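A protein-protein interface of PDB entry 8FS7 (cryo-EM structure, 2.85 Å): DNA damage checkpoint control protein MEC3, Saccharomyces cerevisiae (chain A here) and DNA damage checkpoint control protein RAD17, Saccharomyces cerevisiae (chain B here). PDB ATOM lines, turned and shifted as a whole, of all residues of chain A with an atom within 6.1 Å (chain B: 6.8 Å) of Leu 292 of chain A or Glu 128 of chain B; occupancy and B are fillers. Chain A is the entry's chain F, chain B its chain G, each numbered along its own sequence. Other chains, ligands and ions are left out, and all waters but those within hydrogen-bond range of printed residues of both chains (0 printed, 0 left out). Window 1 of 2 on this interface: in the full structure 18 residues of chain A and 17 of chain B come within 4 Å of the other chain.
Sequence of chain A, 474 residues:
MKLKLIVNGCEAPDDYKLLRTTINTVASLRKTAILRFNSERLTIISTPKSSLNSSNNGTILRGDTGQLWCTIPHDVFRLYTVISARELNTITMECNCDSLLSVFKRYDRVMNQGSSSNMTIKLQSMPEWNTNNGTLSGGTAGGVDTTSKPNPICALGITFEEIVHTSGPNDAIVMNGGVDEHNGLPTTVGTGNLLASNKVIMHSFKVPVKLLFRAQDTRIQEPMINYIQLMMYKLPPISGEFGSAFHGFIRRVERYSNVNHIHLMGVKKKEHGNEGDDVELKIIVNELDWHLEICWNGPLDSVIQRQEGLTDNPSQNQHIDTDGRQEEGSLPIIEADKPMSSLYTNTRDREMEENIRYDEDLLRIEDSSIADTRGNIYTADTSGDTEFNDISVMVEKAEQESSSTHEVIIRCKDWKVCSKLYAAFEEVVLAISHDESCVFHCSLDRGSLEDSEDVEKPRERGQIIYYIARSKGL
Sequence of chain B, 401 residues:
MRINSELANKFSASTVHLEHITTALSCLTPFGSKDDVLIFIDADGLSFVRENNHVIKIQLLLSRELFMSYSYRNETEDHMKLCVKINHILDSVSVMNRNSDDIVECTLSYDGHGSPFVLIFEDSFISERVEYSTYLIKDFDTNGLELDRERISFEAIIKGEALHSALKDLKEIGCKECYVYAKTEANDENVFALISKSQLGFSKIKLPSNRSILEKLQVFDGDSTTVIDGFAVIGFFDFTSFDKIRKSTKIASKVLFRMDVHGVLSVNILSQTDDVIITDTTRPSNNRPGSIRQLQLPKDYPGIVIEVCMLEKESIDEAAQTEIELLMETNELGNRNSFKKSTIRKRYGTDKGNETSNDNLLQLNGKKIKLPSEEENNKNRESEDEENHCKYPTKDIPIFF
NH1 of Arg 255 of chain A lies close to O of Ser 92 of chain B (3.4 Å).
The side-chain carboxylate (OE1) of Glu 128 of chain B lies within salt-bridge range of the guanidinium group (NH1) of Arg 252 of chain A (3.8 Å).
OE2 of Glu 128 of chain B sits at hydrogen-bond distance from OH of Tyr 256 of chain A, 2.7 Å away.
The backbone carbonyl oxygen (O) of Asp 91 of chain B is in hydrogen-bond range of the guanidinium group (NH1) of Arg 255 of chain A.
N of His 291 of chain A sits at hydrogen-bond distance from O of Glu 131 of chain B.
The side-chain carboxylate of Glu 128 of chain B is in salt-bridge range of the guanidinium group of Arg 255 of chain A (2.6 Å).
O of Arg 129 of chain B is in hydrogen-bond range of N of Glu 293 of chain A, at 3.0 Å.
N of Cys 295 of chain A is in hydrogen-bond range of O of Ser 127 of chain B (2.7 Å).
The backbone carbonyl oxygen (O) of Ser 127 of chain B lies close to the backbone carbonyl oxygen (O) of Glu 293 of chain A (3.0 Å).
O of Ile 294 of chain A sits at hydrogen-bond distance from N of Ile 283 of chain A, at 2.7 Å.
The side-chain sulfur (SG) of Cys 295 of chain A lies within hydrogen-bond range of the backbone carbonyl oxygen (O) of Glu 293 of chain A (3.4 Å).
The backbone carbonyl oxygen (O) of Val 285 of chain A is in hydrogen-bond range of the backbone NH (N) of Leu 292 of chain A (3.2 Å).
The backbone NH of Phe 121 of chain B lies within hydrogen-bond range of the backbone carbonyl oxygen of Glu 128 of chain B.
The backbone carbonyl oxygen of Val 130 of chain B is in hydrogen-bond range of the backbone NH of Leu 119 of chain B, 2.7 Å away.
The side-chain carboxylate (OE2) of Glu 131 of chain B is in salt-bridge range of the guanidinium group (NE) of Arg 129 of chain B (3.1 Å).
Among the printed residues, pairs that only touch across the chains: Arg 252 of chain A with Val 95 of chain B (3.9 Å), Arg 252 of chain A with Ile 126 of chain B (3.4 Å), Arg 255 of chain A with Val 95 of chain B (3.4 Å), Tyr 256 of chain A with Asp 91 of chain B (3.5 Å), Tyr 256 of chain A with Ser 92 of chain B (3.9 Å), Tyr 256 of chain A with Val 130 of chain B (3.5 Å), Trp 290 of chain A with Glu 131 of chain B (3.3 Å), Trp 290 of chain A with Tyr 132 of chain B (3.7 Å), His 291 of chain A with Arg 129 of chain B (3.8 Å), His 291 of chain A with Val 130 of chain B (3.4 Å), Leu 292 of chain A with Glu 128 of chain B (3.3 Å), Leu 292 of chain A with Arg 129 of chain B (3.6 Å), Leu 292 of chain A with Val 130 of chain B (3.7 Å), Glu 293 of chain A with Glu 128 of chain B (3.5 Å), Ile 294 of chain A with Ile 126 of chain B (3.9 Å), Ile 294 of chain A with Ser 127 of chain B (3.5 Å) and Cys 295 of chain A with Ile 126 of chain B (3.3 Å).
Of chain B, only Glu 128, Arg 129 and Val 130 come within 4 Å of Leu 292 of chain A.
Glu 128 of chain B touches just these residues of chain A: Arg 252 (3.3 Å), Arg 255 (2.6 Å), Tyr 256 (2.7 Å), Leu 292 (3.3 Å) and Glu 293 (3.5 Å).
Of the printed residues of chain A, Glu 131 of chain B touches Trp 290 (3.3 Å) and His 291 (3.2 Å).
Printed residues of chain A within 4 Å of Ile 126 of chain B: Arg 252 (3.4 Å), Ile 294 (3.9 Å) and Cys 295 (3.3 Å).
Of the printed residues of chain B, Tyr 256 of chain A touches Asp 91 (3.5 Å), Ser 92 (3.9 Å), Glu 128 (2.7 Å) and Val 130 (3.5 Å).
Asn 286 of chain A touches none of the printed residues of chain B.
Phe 121 of chain B touches none of the printed residues of chain A.
The nearest residue of chain A that does not touch Glu 128 of chain B is Ile 294 of chain A (4.1 Å).
The nearest printed residue of chain A that does not touch Glu 131 of chain B is Leu 292 of chain A (5.3 Å).
Of the 15 printed residues of chain B, 10 touch a printed residue of chain A.
Printed residues of chain B that touch a printed residue of chain A: Asp 91, Ser 92, Val 95, Ile 126, Ser 127, Glu 128, Arg 129, Val 130, Glu 131 and Tyr 132.
Hydrophobic or aromatic side chains of chain B that line the printed part of chain A: Val 95, Ile 126, Val 130 and Tyr 132.
Printed residues of chain A that touch a printed residue of chain B: Arg 252, Arg 255, Tyr 256, Trp 290, His 291, Leu 292, Glu 293, Ile 294 and Cys 295.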
ATOM      1  N   ARG A 252      17.159  24.487  31.145  1.00  0.00           N
ATOM      2  CA  ARG A 252      18.551  24.915  31.061  1.00  0.00           C
ATOM      3  C   ARG A 252      18.840  25.746  29.816  1.00  0.00           C
ATOM      4  O   ARG A 252      19.771  26.558  29.831  1.00  0.00           O
ATOM      5  CB  ARG A 252      19.468  23.691  31.097  1.00  0.00           C
ATOM      6  CG  ARG A 252      20.903  23.995  31.484  1.00  0.00           C
ATOM      7  CD  ARG A 252      20.974  24.590  32.880  1.00  0.00           C
ATOM      8  NE  ARG A 252      20.620  23.622  33.911  1.00  0.00           N
ATOM      9  CZ  ARG A 252      21.495  22.862  34.557  1.00  0.00           C
ATOM     10  NH1 ARG A 252      22.790  22.927  34.297  1.00  0.00           N
ATOM     11  NH2 ARG A 252      21.059  22.019  35.487  1.00  0.00           N
ATOM     12  N   VAL A 253      18.070  25.564  28.738  1.00  0.00           N
ATOM     13  CA  VAL A 253      18.280  26.346  27.522  1.00  0.00           C
ATOM     14  C   VAL A 253      17.497  27.652  27.525  1.00  0.00           C
ATOM     15  O   VAL A 253      17.753  28.521  26.675  1.00  0.00           O
ATOM     16  CB  VAL A 253      17.918  25.510  26.276  1.00  0.00           C
ATOM     17  CG1 VAL A 253      16.426  25.593  25.981  1.00  0.00           C
ATOM     18  CG2 VAL A 253      18.744  25.946  25.073  1.00  0.00           C
ATOM     19  N   ARG A 255      17.575  30.008  29.823  1.00  0.00           N
ATOM     20  CA  ARG A 255      18.290  31.090  30.482  1.00  0.00           C
ATOM     21  C   ARG A 255      19.208  31.854  29.536  1.00  0.00           C
ATOM     22  O   ARG A 255      19.845  32.821  29.963  1.00  0.00           O
ATOM     23  CB  ARG A 255      19.095  30.547  31.667  1.00  0.00           C
ATOM     24  CG  ARG A 255      20.053  29.426  31.312  1.00  0.00           C
ATOM     25  CD  ARG A 255      21.262  29.446  32.223  1.00  0.00           C
ATOM     26  NE  ARG A 255      21.861  28.128  32.392  1.00  0.00           N
ATOM     27  CZ  ARG A 255      23.013  27.759  31.851  1.00  0.00           C
ATOM     28  NH1 ARG A 255      23.710  28.579  31.083  1.00  0.00           N
ATOM     29  NH2 ARG A 255      23.480  26.537  32.088  1.00  0.00           N
ATOM     30  N   TYR A 256      19.290  31.443  28.273  1.00  0.00           N
ATOM     31  CA  TYR A 256      20.042  32.173  27.262  1.00  0.00           C
ATOM     32  C   TYR A 256      19.109  33.167  26.581  1.00  0.00           C
ATOM     33  O   TYR A 256      18.025  32.793  26.121  1.00  0.00           O
ATOM     34  CB  TYR A 256      20.651  31.214  26.239  1.00  0.00           C
ATOM     35  CG  TYR A 256      21.794  30.383  26.777  1.00  0.00           C
ATOM     36  CD1 TYR A 256      21.553  29.239  27.528  1.00  0.00           C
ATOM     37  CD2 TYR A 256      23.114  30.737  26.529  1.00  0.00           C
ATOM     38  CE1 TYR A 256      22.594  28.476  28.021  1.00  0.00           C
ATOM     39  CE2 TYR A 256      24.161  29.982  27.020  1.00  0.00           C
ATOM     40  CZ  TYR A 256      23.896  28.851  27.764  1.00  0.00           C
ATOM     41  OH  TYR A 256      24.936  28.094  28.253  1.00  0.00           O
ATOM     42  N   ILE A 283      20.287  18.743  24.138  1.00  0.00           N
ATOM     43  CA  ILE A 283      19.875  20.049  23.640  1.00  0.00           C
ATOM     44  C   ILE A 283      21.110  20.733  23.065  1.00  0.00           C
ATOM     45  O   ILE A 283      22.010  21.137  23.805  1.00  0.00           O
ATOM     46  CB  ILE A 283      19.229  20.894  24.745  1.00  0.00           C
ATOM     47  CG1 ILE A 283      17.982  20.195  25.289  1.00  0.00           C
ATOM     48  CG2 ILE A 283      18.895  22.284  24.233  1.00  0.00           C
ATOM     49  CD1 ILE A 283      17.381  20.870  26.505  1.00  0.00           C
ATOM     50  N   ILE A 284      21.154  20.867  21.741  1.00  0.00           N
ATOM     51  CA  ILE A 284      22.307  21.415  21.038  1.00  0.00           C
ATOM     52  C   ILE A 284      21.896  22.720  20.371  1.00  0.00           C
ATOM     53  O   ILE A 284      20.940  22.748  19.588  1.00  0.00           O
ATOM     54  CB  ILE A 284      22.865  20.423  20.000  1.00  0.00           C
ATOM     55  CG1 ILE A 284      23.514  19.229  20.703  1.00  0.00           C
ATOM     56  CG2 ILE A 284      23.863  21.113  19.081  1.00  0.00           C
ATOM     57  CD1 ILE A 284      24.084  18.197  19.752  1.00  0.00           C
ATOM     58  N   VAL A 285      22.614  23.792  20.683  1.00  0.00           N
ATOM     59  CA  VAL A 285      22.376  25.108  20.093  1.00  0.00           C
ATOM     60  C   VAL A 285      23.688  25.534  19.442  1.00  0.00           C
ATOM     61  O   VAL A 285      24.571  26.104  20.089  1.00  0.00           O
ATOM     62  CB  VAL A 285      21.898  26.136  21.122  1.00  0.00           C
ATOM     63  CG1 VAL A 285      21.315  27.351  20.421  1.00  0.00           C
ATOM     64  CG2 VAL A 285      20.867  25.520  22.054  1.00  0.00           C
ATOM     65  N   ASN A 286      23.819  25.260  18.148  1.00  0.00           N
ATOM     66  CA  ASN A 286      25.027  25.570  17.393  1.00  0.00           C
ATOM     67  C   ASN A 286      24.808  26.847  16.595  1.00  0.00           C
ATOM     68  O   ASN A 286      23.773  27.008  15.942  1.00  0.00           O
ATOM     69  CB  ASN A 286      25.393  24.414  16.460  1.00  0.00           C
ATOM     70  CG  ASN A 286      26.830  24.482  15.977  1.00  0.00           C
ATOM     71  OD1 ASN A 286      27.511  25.492  16.148  1.00  0.00           O
ATOM     72  ND2 ASN A 286      27.299  23.398  15.368  1.00  0.00           N
ATOM     73  N   TRP A 290      29.468  30.198  18.874  1.00  0.00           N
ATOM     74  CA  TRP A 290      29.250  29.588  20.179  1.00  0.00           C
ATOM     75  C   TRP A 290      28.451  28.304  20.011  1.00  0.00           C
ATOM     76  O   TRP A 290      27.617  28.195  19.111  1.00  0.00           O
ATOM     77  CB  TRP A 290      28.540  30.550  21.143  1.00  0.00           C
ATOM     78  CG  TRP A 290      27.055  30.606  20.987  1.00  0.00           C
ATOM     79  CD1 TRP A 290      26.363  31.132  19.939  1.00  0.00           C
ATOM     80  CD2 TRP A 290      26.076  30.114  21.910  1.00  0.00           C
ATOM     81  NE1 TRP A 290      25.011  31.002  20.151  1.00  0.00           N
ATOM     82  CE2 TRP A 290      24.809  30.379  21.354  1.00  0.00           C
ATOM     83  CE3 TRP A 290      26.147  29.476  23.152  1.00  0.00           C
ATOM     84  CZ2 TRP A 290      23.623  30.029  21.997  1.00  0.00           C
ATOM     85  CZ3 TRP A 290      24.971  29.128  23.788  1.00  0.00           C
ATOM     86  CH2 TRP A 290      23.725  29.406  23.210  1.00  0.00           C
ATOM     87  N   HIS A 291      28.722  27.335  20.886  1.00  0.00           N
ATOM     88  CA  HIS A 291      28.100  26.021  20.836  1.00  0.00           C
ATOM     89  C   HIS A 291      27.615  25.638  22.227  1.00  0.00           C
ATOM     90  O   HIS A 291      28.185  26.057  23.237  1.00  0.00           O
ATOM     91  CB  HIS A 291      29.084  24.966  20.301  1.00  0.00           C
ATOM     92  CG  HIS A 291      28.521  23.581  20.247  1.00  0.00           C
ATOM     93  ND1 HIS A 291      27.624  23.178  19.282  1.00  0.00           N
ATOM     94  CD2 HIS A 291      28.728  22.503  21.041  1.00  0.00           C
ATOM     95  CE1 HIS A 291      27.302  21.912  19.483  1.00  0.00           C
ATOM     96  NE2 HIS A 291      27.959  21.479  20.544  1.00  0.00           N
ATOM     97  N   LEU A 292      26.553  24.834  22.270  1.00  0.00           N
ATOM     98  CA  LEU A 292      25.935  24.429  23.526  1.00  0.00           C
ATOM     99  C   LEU A 292      25.613  22.943  23.465  1.00  0.00           C
ATOM    100  O   LEU A 292      25.099  22.461  22.452  1.00  0.00           O
ATOM    101  CB  LEU A 292      24.669  25.250  23.796  1.00  0.00           C
ATOM    102  CG  LEU A 292      23.932  24.998  25.108  1.00  0.00           C
ATOM    103  CD1 LEU A 292      24.869  25.188  26.286  1.00  0.00           C
ATOM    104  CD2 LEU A 292      22.737  25.927  25.223  1.00  0.00           C
ATOM    105  N   GLU A 293      25.923  22.222  24.541  1.00  0.00           N
ATOM    106  CA  GLU A 293      25.855  20.761  24.551  1.00  0.00           C
ATOM    107  C   GLU A 293      25.183  20.272  25.839  1.00  0.00           C
ATOM    108  O   GLU A 293      25.730  19.470  26.597  1.00  0.00           O
ATOM    109  CB  GLU A 293      27.257  20.169  24.357  1.00  0.00           C
ATOM    110  CG  GLU A 293      27.330  18.643  24.206  1.00  0.00           C
ATOM    111  CD  GLU A 293      27.019  18.165  22.800  1.00  0.00           C
ATOM    112  OE1 GLU A 293      27.209  16.961  22.530  1.00  0.00           O
ATOM    113  OE2 GLU A 293      26.591  18.988  21.965  1.00  0.00           O
ATOM    114  N   ILE A 294      23.993  20.803  26.136  1.00  0.00           N
ATOM    115  CA  ILE A 294      23.232  20.302  27.275  1.00  0.00           C
ATOM    116  C   ILE A 294      22.841  18.852  27.026  1.00  0.00           C
ATOM    117  O   ILE A 294      22.277  18.513  25.979  1.00  0.00           O
ATOM    118  CB  ILE A 294      21.992  21.171  27.532  1.00  0.00           C
ATOM    119  CG1 ILE A 294      22.306  22.647  27.298  1.00  0.00           C
ATOM    120  CG2 ILE A 294      21.483  20.962  28.948  1.00  0.00           C
ATOM    121  CD1 ILE A 294      21.118  23.558  27.514  1.00  0.00           C
ATOM    122  N   CYS A 295      23.141  17.988  27.994  1.00  0.00           N
ATOM    123  CA  CYS A 295      22.859  16.565  27.881  1.00  0.00           C
ATOM    124  C   CYS A 295      22.233  16.067  29.176  1.00  0.00           C
ATOM    125  O   CYS A 295      22.511  16.590  30.257  1.00  0.00           O
ATOM    126  CB  CYS A 295      24.130  15.760  27.572  1.00  0.00           C
ATOM    127  SG  CYS A 295      24.926  16.189  26.007  1.00  0.00           S
ATOM    128  N   ASP B  91      24.908  34.346  30.428  1.00  0.00           N
ATOM    129  CA  ASP B  91      23.906  33.284  30.399  1.00  0.00           C
ATOM    130  C   ASP B  91      24.505  31.946  30.823  1.00  0.00           C
ATOM    131  O   ASP B  91      23.825  31.124  31.446  1.00  0.00           O
ATOM    132  CB  ASP B  91      23.270  33.176  29.013  1.00  0.00           C
ATOM    133  CG  ASP B  91      22.598  34.463  28.573  1.00  0.00           C
ATOM    134  OD1 ASP B  91      21.639  34.894  29.246  1.00  0.00           O
ATOM    135  OD2 ASP B  91      23.000  35.022  27.532  1.00  0.00           O
ATOM    136  N   SER B  92      25.778  31.709  30.492  1.00  0.00           N
ATOM    137  CA  SER B  92      26.435  30.479  30.923  1.00  0.00           C
ATOM    138  C   SER B  92      26.607  30.446  32.436  1.00  0.00           C
ATOM    139  O   SER B  92      26.324  29.427  33.076  1.00  0.00           O
ATOM    140  CB  SER B  92      27.787  30.330  30.227  1.00  0.00           C
ATOM    141  OG  SER B  92      28.676  31.361  30.614  1.00  0.00           O
ATOM    142  N   VAL B  95      23.529  29.733  35.828  1.00  0.00           N
ATOM    143  CA  VAL B  95      22.912  28.457  36.183  1.00  0.00           C
ATOM    144  C   VAL B  95      22.072  28.588  37.449  1.00  0.00           C
ATOM    145  O   VAL B  95      21.031  27.931  37.582  1.00  0.00           O
ATOM    146  CB  VAL B  95      23.996  27.368  36.331  1.00  0.00           C
ATOM    147  CG1 VAL B  95      23.366  26.003  36.585  1.00  0.00           C
ATOM    148  CG2 VAL B  95      24.885  27.332  35.101  1.00  0.00           C
ATOM    149  N   LEU B 119      33.290  26.261  28.890  1.00  0.00           N
ATOM    150  CA  LEU B 119      32.666  26.361  30.210  1.00  0.00           C
ATOM    151  C   LEU B 119      31.846  25.092  30.418  1.00  0.00           C
ATOM    152  O   LEU B 119      30.706  24.994  29.955  1.00  0.00           O
ATOM    153  CB  LEU B 119      31.804  27.616  30.325  1.00  0.00           C
ATOM    154  CG  LEU B 119      32.498  28.890  30.811  1.00  0.00           C
ATOM    155  CD1 LEU B 119      32.983  29.714  29.632  1.00  0.00           C
ATOM    156  CD2 LEU B 119      31.564  29.704  31.694  1.00  0.00           C
ATOM    157  N   ILE B 120      32.428  24.121  31.116  1.00  0.00           N
ATOM    158  CA  ILE B 120      31.778  22.840  31.361  1.00  0.00           C
ATOM    159  C   ILE B 120      31.053  22.902  32.697  1.00  0.00           C
ATOM    160  O   ILE B 120      31.644  23.266  33.720  1.00  0.00           O
ATOM    161  CB  ILE B 120      32.800  21.692  31.345  1.00  0.00           C
ATOM    162  CG1 ILE B 120      33.747  21.840  30.155  1.00  0.00           C
ATOM    163  CG2 ILE B 120      32.088  20.350  31.300  1.00  0.00           C
ATOM    164  CD1 ILE B 120      34.851  20.808  30.121  1.00  0.00           C
ATOM    165  N   PHE B 121      29.772  22.544  32.689  1.00  0.00           N
ATOM    166  CA  PHE B 121      28.958  22.501  33.895  1.00  0.00           C
ATOM    167  C   PHE B 121      28.525  21.065  34.144  1.00  0.00           C
ATOM    168  O   PHE B 121      27.947  20.424  33.259  1.00  0.00           O
ATOM    169  CB  PHE B 121      27.736  23.413  33.768  1.00  0.00           C
ATOM    170  CG  PHE B 121      28.074  24.874  33.778  1.00  0.00           C
ATOM    171  CD1 PHE B 121      28.349  25.526  34.967  1.00  0.00           C
ATOM    172  CD2 PHE B 121      28.127  25.594  32.595  1.00  0.00           C
ATOM    173  CE1 PHE B 121      28.664  26.871  34.980  1.00  0.00           C
ATOM    174  CE2 PHE B 121      28.442  26.940  32.601  1.00  0.00           C
ATOM    175  CZ  PHE B 121      28.713  27.577  33.796  1.00  0.00           C
ATOM    176  N   GLU B 122      28.803  20.562  35.344  1.00  0.00           N
ATOM    177  CA  GLU B 122      28.498  19.187  35.710  1.00  0.00           C
ATOM    178  C   GLU B 122      27.532  19.167  36.883  1.00  0.00           C
ATOM    179  O   GLU B 122      27.769  19.824  37.902  1.00  0.00           O
ATOM    180  CB  GLU B 122      29.771  18.410  36.060  1.00  0.00           C
ATOM    181  CG  GLU B 122      30.900  18.595  35.065  1.00  0.00           C
ATOM    182  CD  GLU B 122      30.971  17.468  34.054  1.00  0.00           C
ATOM    183  OE1 GLU B 122      31.179  16.308  34.469  1.00  0.00           O
ATOM    184  OE2 GLU B 122      30.812  17.742  32.847  1.00  0.00           O
ATOM    185  N   ASP B 123      26.450  18.404  36.734  1.00  0.00           N
ATOM    186  CA  ASP B 123      25.469  18.215  37.789  1.00  0.00           C
ATOM    187  C   ASP B 123      25.316  16.752  38.186  1.00  0.00           C
ATOM    188  O   ASP B 123      24.413  16.437  38.965  1.00  0.00           O
ATOM    189  CB  ASP B 123      24.103  18.779  37.347  1.00  0.00           C
ATOM    190  CG  ASP B 123      23.203  19.177  38.519  1.00  0.00           C
ATOM    191  OD1 ASP B 123      22.524  18.310  39.108  1.00  0.00           O
ATOM    192  OD2 ASP B 123      23.161  20.382  38.838  1.00  0.00           O
ATOM    193  N   ILE B 126      23.075  16.221  34.664  1.00  0.00           N
ATOM    194  CA  ILE B 126      23.033  17.047  33.465  1.00  0.00           C
ATOM    195  C   ILE B 126      24.454  17.502  33.163  1.00  0.00           C
ATOM    196  O   ILE B 126      25.133  18.044  34.042  1.00  0.00           O
ATOM    197  CB  ILE B 126      22.107  18.266  33.650  1.00  0.00           C
ATOM    198  CG1 ILE B 126      20.712  17.819  34.090  1.00  0.00           C
ATOM    199  CG2 ILE B 126      22.042  19.097  32.374  1.00  0.00           C
ATOM    200  CD1 ILE B 126      19.889  18.916  34.717  1.00  0.00           C
ATOM    201  N   SER B 127      24.904  17.281  31.931  1.00  0.00           N
ATOM    202  CA  SER B 127      26.218  17.731  31.484  1.00  0.00           C
ATOM    203  C   SER B 127      26.026  18.768  30.391  1.00  0.00           C
ATOM    204  O   SER B 127      25.367  18.497  29.382  1.00  0.00           O
ATOM    205  CB  SER B 127      27.065  16.561  30.978  1.00  0.00           C
ATOM    206  OG  SER B 127      27.315  15.625  32.013  1.00  0.00           O
ATOM    207  N   GLU B 128      26.595  19.954  30.593  1.00  0.00           N
ATOM    208  CA  GLU B 128      26.488  21.052  29.640  1.00  0.00           C
ATOM    209  C   GLU B 128      27.883  21.571  29.325  1.00  0.00           C
ATOM    210  O   GLU B 128      28.639  21.921  30.238  1.00  0.00           O
ATOM    211  CB  GLU B 128      25.605  22.173  30.190  1.00  0.00           C
ATOM    212  CG  GLU B 128      25.795  23.509  29.494  1.00  0.00           C
ATOM    213  CD  GLU B 128      24.923  24.599  30.082  1.00  0.00           C
ATOM    214  OE1 GLU B 128      24.182  24.312  31.045  1.00  0.00           O
ATOM    215  OE2 GLU B 128      24.976  25.742  29.583  1.00  0.00           O
ATOM    216  N   ARG B 129      28.219  21.619  28.039  1.00  0.00           N
ATOM    217  CA  ARG B 129      29.495  22.148  27.571  1.00  0.00           C
ATOM    218  C   ARG B 129      29.223  23.337  26.663  1.00  0.00           C
ATOM    219  O   ARG B 129      28.539  23.198  25.644  1.00  0.00           O
ATOM    220  CB  ARG B 129      30.300  21.078  26.832  1.00  0.00           C
ATOM    221  CG  ARG B 129      31.634  21.571  26.296  1.00  0.00           C
ATOM    222  CD  ARG B 129      32.238  20.581  25.312  1.00  0.00           C
ATOM    223  NE  ARG B 129      33.695  20.646  25.298  1.00  0.00           N
ATOM    224  CZ  ARG B 129      34.481  20.061  26.191  1.00  0.00           C
ATOM    225  NH1 ARG B 129      33.983  19.342  27.183  1.00  0.00           N
ATOM    226  NH2 ARG B 129      35.799  20.197  26.084  1.00  0.00           N
ATOM    227  N   VAL B 130      29.756  24.500  27.031  1.00  0.00           N
ATOM    228  CA  VAL B 130      29.588  25.727  26.264  1.00  0.00           C
ATOM    229  C   VAL B 130      30.959  26.188  25.797  1.00  0.00           C
ATOM    230  O   VAL B 130      31.868  26.375  26.614  1.00  0.00           O
ATOM    231  CB  VAL B 130      28.896  26.828  27.088  1.00  0.00           C
ATOM    232  CG1 VAL B 130      28.176  27.800  26.168  1.00  0.00           C
ATOM    233  CG2 VAL B 130      27.936  26.223  28.100  1.00  0.00           C
ATOM    234  N   GLU B 131      31.106  26.375  24.488  1.00  0.00           N
ATOM    235  CA  GLU B 131      32.353  26.822  23.886  1.00  0.00           C
ATOM    236  C   GLU B 131      32.151  28.189  23.251  1.00  0.00           C
ATOM    237  O   GLU B 131      31.141  28.430  22.584  1.00  0.00           O
ATOM    238  CB  GLU B 131      32.848  25.822  22.835  1.00  0.00           C
ATOM    239  CG  GLU B 131      33.088  24.423  23.375  1.00  0.00           C
ATOM    240  CD  GLU B 131      33.617  23.474  22.318  1.00  0.00           C
ATOM    241  OE1 GLU B 131      33.671  23.870  21.135  1.00  0.00           O
ATOM    242  OE2 GLU B 131      33.979  22.331  22.671  1.00  0.00           O
ATOM    243  N   TYR B 132      33.114  29.084  23.463  1.00  0.00           N
ATOM    244  CA  TYR B 132      33.064  30.436  22.925  1.00  0.00           C
ATOM    245  C   TYR B 132      34.320  30.708  22.113  1.00  0.00           C
ATOM    246  O   TYR B 132      35.436  30.576  22.627  1.00  0.00           O
ATOM    247  CB  TYR B 132      32.929  31.472  24.044  1.00  0.00           C
ATOM    248  CG  TYR B 132      31.663  31.333  24.852  1.00  0.00           C
ATOM    249  CD1 TYR B 132      30.424  31.294  24.228  1.00  0.00           C
ATOM    250  CD2 TYR B 132      31.704  31.251  26.236  1.00  0.00           C
ATOM    251  CE1 TYR B 132      29.263  31.167  24.960  1.00  0.00           C
ATOM    252  CE2 TYR B 132      30.546  31.127  26.978  1.00  0.00           C
ATOM    253  CZ  TYR B 132      29.328  31.087  26.334  1.00  0.00           C
ATOM    254  OH  TYR B 132      28.169  30.964  27.064  1.00  0.00           O
